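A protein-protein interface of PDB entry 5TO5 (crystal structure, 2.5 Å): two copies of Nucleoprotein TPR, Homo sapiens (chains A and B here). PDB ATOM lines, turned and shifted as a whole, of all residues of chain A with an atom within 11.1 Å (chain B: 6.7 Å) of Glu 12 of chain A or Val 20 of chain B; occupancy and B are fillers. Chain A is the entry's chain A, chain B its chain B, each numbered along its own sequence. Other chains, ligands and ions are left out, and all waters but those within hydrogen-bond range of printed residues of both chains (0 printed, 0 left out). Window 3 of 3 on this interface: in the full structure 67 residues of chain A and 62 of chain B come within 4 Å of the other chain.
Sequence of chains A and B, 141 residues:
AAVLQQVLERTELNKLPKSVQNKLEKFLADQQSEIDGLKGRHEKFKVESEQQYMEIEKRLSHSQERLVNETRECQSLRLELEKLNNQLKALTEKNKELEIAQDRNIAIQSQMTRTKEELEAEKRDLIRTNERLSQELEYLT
The side-chain carboxylate (OE2) of Glu 9 of chain A is in salt-bridge range of the side-chain amino group (NZ) of Lys 23 of chain B, at 3.0 Å.
The side-chain carboxylate (OE1) of Glu 12 of chain A is in salt-bridge range of the side-chain amino group (NZ) of Lys 23 of chain B (3.1 Å).
Hydrophobic or aromatic side chains of chain A that line the printed part of chain B: Leu 4, Val 7, Leu 8, Leu 16 and Leu 24.
Along chain A the printed residues that touch a printed residue of chain B span positions 4 to 24.
Of the 11 printed residues of chain B, 4 touch a printed residue of chain A.
Hydrophobic or aromatic side chains of chain B within 4 Å of the printed part of chain A: Leu 16, Val 20 and Leu 24.
Of the printed residues of chain B, Leu 4 of chain A touches Leu 24.
Printed residues of chain B within 4 Å of Val 7 of chain A: Leu 24 (3.8 Å).
Of chain B, only Val 20 (3.6 Å) and Lys 23 (3.1 Å) come within 4 Å of Glu 12 of chain A.
Printed residues of chain B within 4 Å of Leu 16 of chain A: Leu 16 (3.5 Å).
Printed residues of chain B within 4 Å of Leu 24 of chain A: Leu 24 (3.7 Å).
No residue of chain A comes within 4 Å of Pro 17 of chain B.
No residue of chain A comes within 4 Å of Ser 19 of chain B.
No residue of chain A comes within 4 Å of Gln 21 of chain B.
Lys 23 of chain B touches just these residues of chain A: Glu 9 and Glu 12.
Leu 24 of chain B touches just these residues of chain A: Leu 4 (3.9 Å), Val 7 (3.8 Å), Leu 8 (3.96 Å) and Leu 24 (3.7 Å).
The nearest residue of chain B that does not touch Glu 12 of chain A is Ser 19 of chain B (4.3 Å).
The nearest residue of chain A that does not touch Val 20 of chain B is Leu 16 of chain A (4.7 Å).
The nearest printed residue of chain B that does not touch Leu 16 of chain A is Val 20 of chain B (4.7 Å).
Among the printed residues, merely in contact across the chains: Leu 4 of chain A with Leu 24 of chain B, Val 7 of chain A with Leu 24 of chain B, Leu 8 of chain A with Val 20 of chain B, Leu 8 of chain A with Leu 24 of chain B, Glu 12 of chain A with Val 20 of chain B, Leu 16 of chain A with Leu 16 of chain B and Leu 24 of chain A with Leu 24 of chain B.
The backbone carbonyl oxygen (O) of Leu 16 of chain A is in hydrogen-bond range of the side-chain amide nitrogen (NE2) of Gln 21 of chain A, 2.6 Å away.
OE1 of Glu 9 of chain A sits at hydrogen-bond distance from OG1 of Thr 11 of chain A (3.4 Å).
The side-chain carboxylate (OE1) of Glu 12 of chain A lies within hydrogen-bond range of the backbone NH (N) of Glu 9 of chain A (3.3 Å).
NE2 of Gln 21 of chain B is in hydrogen-bond range of O of Leu 16 of chain B, at 2.8 Å.
Leu 4 of chain A touches Leu 24 of chain B, but with the chains exchanged Leu 24 of chain A does not touch Leu 4 of chain B (4.01 Å).
Leu 16 of chain A touches its own counterpart, Leu 16 of chain B.
Leu 24 of chain B touches its own counterpart, Leu 24 of chain A.
Positions printed for both chains: 4, 16, 17, 18, 20, 21 and 24.
Of the 9 pairs that touch across the chains among the printed residues, 2 have their exchanged pair printed and touching as well.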
ATOM      1  N   VAL A   3       5.235 -19.173  -3.590  1.00  0.00           N
ATOM      2  CA  VAL A   3       4.381 -20.171  -4.218  1.00  0.00           C
ATOM      3  C   VAL A   3       3.059 -20.337  -3.465  1.00  0.00           C
ATOM      4  O   VAL A   3       2.043 -20.720  -4.050  1.00  0.00           O
ATOM      5  CB  VAL A   3       5.107 -21.526  -4.310  1.00  0.00           C
ATOM      6  CG1 VAL A   3       4.361 -22.472  -5.233  1.00  0.00           C
ATOM      7  CG2 VAL A   3       6.524 -21.319  -4.815  1.00  0.00           C
ATOM      8  N   LEU A   4       3.076 -20.039  -2.169  1.00  0.00           N
ATOM      9  CA  LEU A   4       1.921 -20.292  -1.316  1.00  0.00           C
ATOM     10  C   LEU A   4       0.796 -19.294  -1.551  1.00  0.00           C
ATOM     11  O   LEU A   4      -0.381 -19.637  -1.441  1.00  0.00           O
ATOM     12  CB  LEU A   4       2.334 -20.270   0.153  1.00  0.00           C
ATOM     13  CG  LEU A   4       1.508 -21.151   1.092  1.00  0.00           C
ATOM     14  CD1 LEU A   4       1.329 -22.539   0.495  1.00  0.00           C
ATOM     15  CD2 LEU A   4       2.203 -21.243   2.436  1.00  0.00           C
ATOM     16  N   GLN A   5       1.153 -18.057  -1.872  1.00  0.00           N
ATOM     17  CA  GLN A   5       0.144 -17.045  -2.145  1.00  0.00           C
ATOM     18  C   GLN A   5      -0.529 -17.328  -3.490  1.00  0.00           C
ATOM     19  O   GLN A   5      -1.587 -16.773  -3.787  1.00  0.00           O
ATOM     20  CB  GLN A   5       0.764 -15.648  -2.130  1.00  0.00           C
ATOM     21  CG  GLN A   5       1.572 -15.345  -3.367  1.00  0.00           C
ATOM     22  CD  GLN A   5       2.609 -14.263  -3.156  1.00  0.00           C
ATOM     23  OE1 GLN A   5       2.596 -13.554  -2.153  1.00  0.00           O
ATOM     24  NE2 GLN A   5       3.523 -14.137  -4.108  1.00  0.00           N
ATOM     25  N   GLN A   6       0.087 -18.192  -4.298  1.00  0.00           N
ATOM     26  CA  GLN A   6      -0.500 -18.603  -5.570  1.00  0.00           C
ATOM     27  C   GLN A   6      -1.632 -19.610  -5.374  1.00  0.00           C
ATOM     28  O   GLN A   6      -2.672 -19.525  -6.026  1.00  0.00           O
ATOM     29  CB  GLN A   6       0.556 -19.217  -6.493  1.00  0.00           C
ATOM     30  CG  GLN A   6       1.822 -18.402  -6.708  1.00  0.00           C
ATOM     31  CD  GLN A   6       2.844 -19.160  -7.537  1.00  0.00           C
ATOM     32  OE1 GLN A   6       2.504 -20.118  -8.231  1.00  0.00           O
ATOM     33  NE2 GLN A   6       4.103 -18.746  -7.458  1.00  0.00           N
ATOM     34  N   VAL A   7      -1.418 -20.582  -4.492  1.00  0.00           N
ATOM     35  CA  VAL A   7      -2.400 -21.642  -4.294  1.00  0.00           C
ATOM     36  C   VAL A   7      -3.549 -21.212  -3.382  1.00  0.00           C
ATOM     37  O   VAL A   7      -4.711 -21.489  -3.674  1.00  0.00           O
ATOM     38  CB  VAL A   7      -1.731 -22.929  -3.743  1.00  0.00           C
ATOM     39  CG1 VAL A   7      -0.694 -23.415  -4.717  1.00  0.00           C
ATOM     40  CG2 VAL A   7      -1.078 -22.692  -2.394  1.00  0.00           C
ATOM     41  N   LEU A   8      -3.234 -20.510  -2.297  1.00  0.00           N
ATOM     42  CA  LEU A   8      -4.256 -20.103  -1.337  1.00  0.00           C
ATOM     43  C   LEU A   8      -4.615 -18.630  -1.484  1.00  0.00           C
ATOM     44  O   LEU A   8      -3.959 -17.892  -2.222  1.00  0.00           O
ATOM     45  CB  LEU A   8      -3.782 -20.368   0.096  1.00  0.00           C
ATOM     46  CG  LEU A   8      -3.398 -21.787   0.521  1.00  0.00           C
ATOM     47  CD1 LEU A   8      -2.753 -21.753   1.893  1.00  0.00           C
ATOM     48  CD2 LEU A   8      -4.613 -22.702   0.529  1.00  0.00           C
ATOM     49  N   GLU A   9      -5.625 -18.194  -0.735  1.00  0.00           N
ATOM     50  CA  GLU A   9      -6.042 -16.799  -0.765  1.00  0.00           C
ATOM     51  C   GLU A   9      -5.350 -16.047   0.355  1.00  0.00           C
ATOM     52  O   GLU A   9      -4.703 -16.662   1.199  1.00  0.00           O
ATOM     53  CB  GLU A   9      -7.557 -16.687  -0.613  1.00  0.00           C
ATOM     54  CG  GLU A   9      -8.324 -17.510  -1.621  1.00  0.00           C
ATOM     55  CD  GLU A   9      -9.700 -17.906  -1.126  1.00  0.00           C
ATOM     56  OE1 GLU A   9     -10.218 -17.244  -0.202  1.00  0.00           O
ATOM     57  OE2 GLU A   9     -10.259 -18.887  -1.656  1.00  0.00           O
ATOM     58  N   ARG A  10      -5.528 -14.732   0.403  1.00  0.00           N
ATOM     59  CA  ARG A  10      -4.882 -13.932   1.436  1.00  0.00           C
ATOM     60  C   ARG A  10      -5.557 -14.149   2.780  1.00  0.00           C
ATOM     61  O   ARG A  10      -4.950 -13.951   3.829  1.00  0.00           O
ATOM     62  CB  ARG A  10      -4.897 -12.445   1.068  1.00  0.00           C
ATOM     63  CG  ARG A  10      -3.740 -12.006   0.176  1.00  0.00           C
ATOM     64  CD  ARG A  10      -2.411 -12.048   0.920  1.00  0.00           C
ATOM     65  NE  ARG A  10      -1.289 -11.698   0.052  1.00  0.00           N
ATOM     66  CZ  ARG A  10      -0.034 -11.562   0.469  1.00  0.00           C
ATOM     67  NH1 ARG A  10       0.266 -11.741   1.749  1.00  0.00           N
ATOM     68  NH2 ARG A  10       0.924 -11.244  -0.393  1.00  0.00           N
ATOM     69  N   THR A  11      -6.815 -14.567   2.749  1.00  0.00           N
ATOM     70  CA  THR A  11      -7.550 -14.800   3.983  1.00  0.00           C
ATOM     71  C   THR A  11      -7.180 -16.136   4.615  1.00  0.00           C
ATOM     72  O   THR A  11      -7.067 -16.240   5.834  1.00  0.00           O
ATOM     73  CB  THR A  11      -9.068 -14.767   3.759  1.00  0.00           C
ATOM     74  OG1 THR A  11      -9.436 -15.775   2.807  1.00  0.00           O
ATOM     75  CG2 THR A  11      -9.509 -13.404   3.248  1.00  0.00           C
ATOM     76  N   GLU A  12      -7.015 -17.166   3.791  1.00  0.00           N
ATOM     77  CA  GLU A  12      -6.734 -18.493   4.326  1.00  0.00           C
ATOM     78  C   GLU A  12      -5.241 -18.781   4.462  1.00  0.00           C
ATOM     79  O   GLU A  12      -4.849 -19.710   5.172  1.00  0.00           O
ATOM     80  CB  GLU A  12      -7.398 -19.565   3.460  1.00  0.00           C
ATOM     81  CG  GLU A  12      -7.190 -19.407   1.966  1.00  0.00           C
ATOM     82  CD  GLU A  12      -8.110 -20.310   1.170  1.00  0.00           C
ATOM     83  OE1 GLU A  12      -7.849 -20.518  -0.031  1.00  0.00           O
ATOM     84  OE2 GLU A  12      -9.098 -20.807   1.749  1.00  0.00           O
ATOM     85  N   LEU A  13      -4.410 -17.968   3.817  1.00  0.00           N
ATOM     86  CA  LEU A  13      -2.972 -18.083   3.998  1.00  0.00           C
ATOM     87  C   LEU A  13      -2.610 -17.475   5.342  1.00  0.00           C
ATOM     88  O   LEU A  13      -1.746 -17.982   6.054  1.00  0.00           O
ATOM     89  CB  LEU A  13      -2.209 -17.391   2.866  1.00  0.00           C
ATOM     90  CG  LEU A  13      -0.691 -17.244   2.985  1.00  0.00           C
ATOM     91  CD1 LEU A  13      -0.045 -18.574   3.333  1.00  0.00           C
ATOM     92  CD2 LEU A  13      -0.113 -16.704   1.687  1.00  0.00           C
ATOM     93  N   ASN A  14      -3.295 -16.395   5.697  1.00  0.00           N
ATOM     94  CA  ASN A  14      -3.001 -15.708   6.944  1.00  0.00           C
ATOM     95  C   ASN A  14      -3.535 -16.472   8.155  1.00  0.00           C
ATOM     96  O   ASN A  14      -3.162 -16.180   9.291  1.00  0.00           O
ATOM     97  CB  ASN A  14      -3.559 -14.285   6.909  1.00  0.00           C
ATOM     98  CG  ASN A  14      -2.841 -13.402   5.900  1.00  0.00           C
ATOM     99  OD1 ASN A  14      -1.673 -13.626   5.583  1.00  0.00           O
ATOM    100  ND2 ASN A  14      -3.539 -12.396   5.391  1.00  0.00           N
ATOM    101  N   LYS A  15      -4.394 -17.459   7.909  1.00  0.00           N
ATOM    102  CA  LYS A  15      -4.883 -18.327   8.977  1.00  0.00           C
ATOM    103  C   LYS A  15      -3.877 -19.431   9.307  1.00  0.00           C
ATOM    104  O   LYS A  15      -4.034 -20.143  10.297  1.00  0.00           O
ATOM    105  CB  LYS A  15      -6.234 -18.946   8.601  1.00  0.00           C
ATOM    106  CG  LYS A  15      -7.410 -17.977   8.621  1.00  0.00           C
ATOM    107  CD  LYS A  15      -8.676 -18.648   8.102  1.00  0.00           C
ATOM    108  CE  LYS A  15      -9.855 -17.682   8.050  1.00  0.00           C
ATOM    109  NZ  LYS A  15     -10.282 -17.221   9.400  1.00  0.00           N
ATOM    110  N   LEU A  16      -2.851 -19.576   8.474  1.00  0.00           N
ATOM    111  CA  LEU A  16      -1.808 -20.559   8.739  1.00  0.00           C
ATOM    112  C   LEU A  16      -0.730 -19.977   9.651  1.00  0.00           C
ATOM    113  O   LEU A  16      -0.276 -18.855   9.440  1.00  0.00           O
ATOM    114  CB  LEU A  16      -1.181 -21.046   7.431  1.00  0.00           C
ATOM    115  CG  LEU A  16      -2.059 -21.742   6.389  1.00  0.00           C
ATOM    116  CD1 LEU A  16      -1.256 -21.988   5.128  1.00  0.00           C
ATOM    117  CD2 LEU A  16      -2.602 -23.045   6.931  1.00  0.00           C
ATOM    118  N   PRO A  17      -0.322 -20.740  10.679  1.00  0.00           N
ATOM    119  CA  PRO A  17       0.818 -20.347  11.517  1.00  0.00           C
ATOM    120  C   PRO A  17       2.079 -20.096  10.700  1.00  0.00           C
ATOM    121  O   PRO A  17       2.194 -20.622   9.592  1.00  0.00           O
ATOM    122  CB  PRO A  17       1.002 -21.554  12.441  1.00  0.00           C
ATOM    123  CG  PRO A  17      -0.364 -22.102  12.589  1.00  0.00           C
ATOM    124  CD  PRO A  17      -1.057 -21.879  11.262  1.00  0.00           C
ATOM    125  N   LYS A  18       2.987 -19.278  11.226  1.00  0.00           N
ATOM    126  CA  LYS A  18       4.244 -18.996  10.541  1.00  0.00           C
ATOM    127  C   LYS A  18       4.982 -20.297  10.236  1.00  0.00           C
ATOM    128  O   LYS A  18       5.416 -20.519   9.109  1.00  0.00           O
ATOM    129  CB  LYS A  18       5.137 -18.075  11.379  1.00  0.00           C
ATOM    130  CG  LYS A  18       6.055 -17.181  10.550  1.00  0.00           C
ATOM    131  CD  LYS A  18       7.220 -16.633  11.366  1.00  0.00           C
ATOM    132  CE  LYS A  18       6.748 -16.003  12.665  1.00  0.00           C
ATOM    133  NZ  LYS A  18       7.885 -15.457  13.458  1.00  0.00           N
ATOM    134  N   VAL A  20       3.951 -23.413   9.986  1.00  0.00           N
ATOM    135  CA  VAL A  20       3.239 -24.127   8.941  1.00  0.00           C
ATOM    136  C   VAL A  20       3.482 -23.523   7.558  1.00  0.00           C
ATOM    137  O   VAL A  20       3.712 -24.259   6.595  1.00  0.00           O
ATOM    138  CB  VAL A  20       1.730 -24.149   9.244  1.00  0.00           C
ATOM    139  CG1 VAL A  20       0.951 -24.748   8.089  1.00  0.00           C
ATOM    140  CG2 VAL A  20       1.473 -24.923  10.531  1.00  0.00           C
ATOM    141  N   GLN A  21       3.443 -22.194   7.454  1.00  0.00           N
ATOM    142  CA  GLN A  21       3.697 -21.548   6.168  1.00  0.00           C
ATOM    143  C   GLN A  21       5.126 -21.857   5.727  1.00  0.00           C
ATOM    144  O   GLN A  21       5.357 -22.265   4.592  1.00  0.00           O
ATOM    145  CB  GLN A  21       3.459 -20.030   6.239  1.00  0.00           C
ATOM    146  CG  GLN A  21       2.005 -19.629   6.496  1.00  0.00           C
ATOM    147  CD  GLN A  21       1.786 -18.117   6.591  1.00  0.00           C
ATOM    148  OE1 GLN A  21       2.526 -17.329   6.004  1.00  0.00           O
ATOM    149  NE2 GLN A  21       0.758 -17.714   7.334  1.00  0.00           N
ATOM    150  N   LEU A  24       5.514 -25.485   4.311  1.00  0.00           N
ATOM    151  CA  LEU A  24       4.900 -25.626   2.993  1.00  0.00           C
ATOM    152  C   LEU A  24       5.731 -24.938   1.913  1.00  0.00           C
ATOM    153  O   LEU A  24       6.061 -25.552   0.902  1.00  0.00           O
ATOM    154  CB  LEU A  24       3.472 -25.071   3.004  1.00  0.00           C
ATOM    155  CG  LEU A  24       2.472 -25.897   3.821  1.00  0.00           C
ATOM    156  CD1 LEU A  24       1.198 -25.112   4.084  1.00  0.00           C
ATOM    157  CD2 LEU A  24       2.160 -27.204   3.104  1.00  0.00           C
ATOM    158  N   LEU A  28       7.397 -26.613  -1.251  1.00  0.00           N
ATOM    159  CA  LEU A  28       6.951 -26.199  -2.578  1.00  0.00           C
ATOM    160  C   LEU A  28       8.116 -25.623  -3.376  1.00  0.00           C
ATOM    161  O   LEU A  28       8.189 -25.793  -4.588  1.00  0.00           O
ATOM    162  CB  LEU A  28       5.802 -25.183  -2.488  1.00  0.00           C
ATOM    163  CG  LEU A  28       4.378 -25.758  -2.464  1.00  0.00           C
ATOM    164  CD1 LEU A  28       4.147 -26.636  -1.245  1.00  0.00           C
ATOM    165  CD2 LEU A  28       3.332 -24.658  -2.525  1.00  0.00           C
ATOM    166  N   LEU B   4       0.367 -34.045   1.760  1.00  0.00           N
ATOM    167  CA  LEU B   4       0.336 -33.129   2.904  1.00  0.00           C
ATOM    168  C   LEU B   4       0.905 -33.751   4.177  1.00  0.00           C
ATOM    169  O   LEU B   4       1.178 -33.052   5.150  1.00  0.00           O
ATOM    170  CB  LEU B   4      -1.090 -32.651   3.175  1.00  0.00           C
ATOM    171  CG  LEU B   4      -1.498 -31.275   2.645  1.00  0.00           C
ATOM    172  CD1 LEU B   4      -2.883 -30.918   3.148  1.00  0.00           C
ATOM    173  CD2 LEU B   4      -0.498 -30.210   3.062  1.00  0.00           C
ATOM    174  N   LEU B  16      -5.997 -27.640   9.760  1.00  0.00           N
ATOM    175  CA  LEU B  16      -6.331 -26.908   8.543  1.00  0.00           C
ATOM    176  C   LEU B  16      -7.735 -27.271   8.071  1.00  0.00           C
ATOM    177  O   LEU B  16      -8.139 -28.431   8.156  1.00  0.00           O
ATOM    178  CB  LEU B  16      -5.318 -27.198   7.431  1.00  0.00           C
ATOM    179  CG  LEU B  16      -3.820 -27.227   7.751  1.00  0.00           C
ATOM    180  CD1 LEU B  16      -3.021 -27.336   6.460  1.00  0.00           C
ATOM    181  CD2 LEU B  16      -3.389 -26.012   8.555  1.00  0.00           C
ATOM    182  N   PRO B  17      -8.487 -26.277   7.572  1.00  0.00           N
ATOM    183  CA  PRO B  17      -9.818 -26.544   7.016  1.00  0.00           C
ATOM    184  C   PRO B  17      -9.744 -27.512   5.842  1.00  0.00           C
ATOM    185  O   PRO B  17      -8.680 -27.658   5.244  1.00  0.00           O
ATOM    186  CB  PRO B  17     -10.298 -25.161   6.565  1.00  0.00           C
ATOM    187  CG  PRO B  17      -9.527 -24.206   7.406  1.00  0.00           C
ATOM    188  CD  PRO B  17      -8.178 -24.838   7.593  1.00  0.00           C
ATOM    189  N   LYS B  18     -10.852 -28.166   5.519  1.00  0.00           N
ATOM    190  CA  LYS B  18     -10.839 -29.180   4.474  1.00  0.00           C
ATOM    191  C   LYS B  18     -10.581 -28.585   3.095  1.00  0.00           C
ATOM    192  O   LYS B  18      -9.869 -29.180   2.281  1.00  0.00           O
ATOM    193  CB  LYS B  18     -12.151 -29.958   4.457  1.00  0.00           C
ATOM    194  CG  LYS B  18     -12.010 -31.324   3.822  1.00  0.00           C
ATOM    195  CD  LYS B  18     -11.130 -32.211   4.687  1.00  0.00           C
ATOM    196  CE  LYS B  18     -10.754 -33.500   3.980  1.00  0.00           C
ATOM    197  NZ  LYS B  18      -9.699 -33.284   2.953  1.00  0.00           N
ATOM    198  N   SER B  19     -11.160 -27.417   2.831  1.00  0.00           N
ATOM    199  CA  SER B  19     -10.978 -26.767   1.540  1.00  0.00           C
ATOM    200  C   SER B  19      -9.517 -26.387   1.340  1.00  0.00           C
ATOM    201  O   SER B  19      -8.971 -26.530   0.249  1.00  0.00           O
ATOM    202  CB  SER B  19     -11.861 -25.528   1.426  1.00  0.00           C
ATOM    203  OG  SER B  19     -11.344 -24.471   2.212  1.00  0.00           O
ATOM    204  N   VAL B  20      -8.888 -25.904   2.405  1.00  0.00           N
ATOM    205  CA  VAL B  20      -7.480 -25.543   2.357  1.00  0.00           C
ATOM    206  C   VAL B  20      -6.618 -26.784   2.120  1.00  0.00           C
ATOM    207  O   VAL B  20      -5.713 -26.765   1.287  1.00  0.00           O
ATOM    208  CB  VAL B  20      -7.042 -24.824   3.649  1.00  0.00           C
ATOM    209  CG1 VAL B  20      -5.533 -24.685   3.697  1.00  0.00           C
ATOM    210  CG2 VAL B  20      -7.707 -23.455   3.740  1.00  0.00           C
ATOM    211  N   GLN B  21      -6.916 -27.865   2.836  1.00  0.00           N
ATOM    212  CA  GLN B  21      -6.199 -29.124   2.648  1.00  0.00           C
ATOM    213  C   GLN B  21      -6.320 -29.627   1.213  1.00  0.00           C
ATOM    214  O   GLN B  21      -5.330 -30.046   0.619  1.00  0.00           O
ATOM    215  CB  GLN B  21      -6.706 -30.198   3.611  1.00  0.00           C
ATOM    216  CG  GLN B  21      -6.283 -29.999   5.054  1.00  0.00           C
ATOM    217  CD  GLN B  21      -6.714 -31.148   5.944  1.00  0.00           C
ATOM    218  OE1 GLN B  21      -6.776 -32.300   5.507  1.00  0.00           O
ATOM    219  NE2 GLN B  21      -7.019 -30.839   7.200  1.00  0.00           N
ATOM    220  N   ASN B  22      -7.531 -29.583   0.660  1.00  0.00           N
ATOM    221  CA  ASN B  22      -7.751 -30.013  -0.719  1.00  0.00           C
ATOM    222  C   ASN B  22      -6.977 -29.163  -1.718  1.00  0.00           C
ATOM    223  O   ASN B  22      -6.469 -29.670  -2.715  1.00  0.00           O
ATOM    224  CB  ASN B  22      -9.241 -29.973  -1.070  1.00  0.00           C
ATOM    225  CG  ASN B  22     -10.049 -31.007  -0.313  1.00  0.00           C
ATOM    226  OD1 ASN B  22      -9.525 -32.037   0.113  1.00  0.00           O
ATOM    227  ND2 ASN B  22     -11.341 -30.739  -0.149  1.00  0.00           N
ATOM    228  N   LYS B  23      -6.893 -27.866  -1.444  1.00  0.00           N
ATOM    229  CA  LYS B  23      -6.226 -26.935  -2.348  1.00  0.00           C
ATOM    230  C   LYS B  23      -4.721 -27.182  -2.385  1.00  0.00           C
ATOM    231  O   LYS B  23      -4.118 -27.206  -3.461  1.00  0.00           O
ATOM    232  CB  LYS B  23      -6.521 -25.489  -1.946  1.00  0.00           C
ATOM    233  CG  LYS B  23      -7.901 -25.011  -2.383  1.00  0.00           C
ATOM    234  CD  LYS B  23      -8.271 -23.660  -1.780  1.00  0.00           C
ATOM    235  CE  LYS B  23      -9.692 -23.273  -2.168  1.00  0.00           C
ATOM    236  NZ  LYS B  23     -10.074 -21.899  -1.730  1.00  0.00           N
ATOM    237  N   LEU B  24      -4.122 -27.378  -1.214  1.00  0.00           N
ATOM    238  CA  LEU B  24      -2.697 -27.674  -1.125  1.00  0.00           C
ATOM    239  C   LEU B  24      -2.396 -29.047  -1.700  1.00  0.00           C
ATOM    240  O   LEU B  24      -1.438 -29.221  -2.449  1.00  0.00           O
ATOM    241  CB  LEU B  24      -2.213 -27.621   0.322  1.00  0.00           C
ATOM    242  CG  LEU B  24      -2.303 -26.302   1.083  1.00  0.00           C
ATOM    243  CD1 LEU B  24      -1.849 -26.515   2.516  1.00  0.00           C
ATOM    244  CD2 LEU B  24      -1.465 -25.236   0.400  1.00  0.00           C
ATOM    245  N   GLU B  25      -3.222 -30.020  -1.327  1.00  0.00           N
ATOM    246  CA  GLU B  25      -3.009 -31.405  -1.727  1.00  0.00           C
ATOM    247  C   GLU B  25      -3.038 -31.551  -3.242  1.00  0.00           C
ATOM    248  O   GLU B  25      -2.223 -32.273  -3.819  1.00  0.00           O
ATOM    249  CB  GLU B  25      -4.061 -32.315  -1.092  1.00  0.00           C
ATOM    250  CG  GLU B  25      -3.902 -33.785  -1.435  1.00  0.00           C
ATOM    251  CD  GLU B  25      -2.616 -34.380  -0.897  1.00  0.00           C
ATOM    252  OE1 GLU B  25      -2.032 -35.247  -1.580  1.00  0.00           O
ATOM    253  OE2 GLU B  25      -2.192 -33.986   0.207  1.00  0.00           O
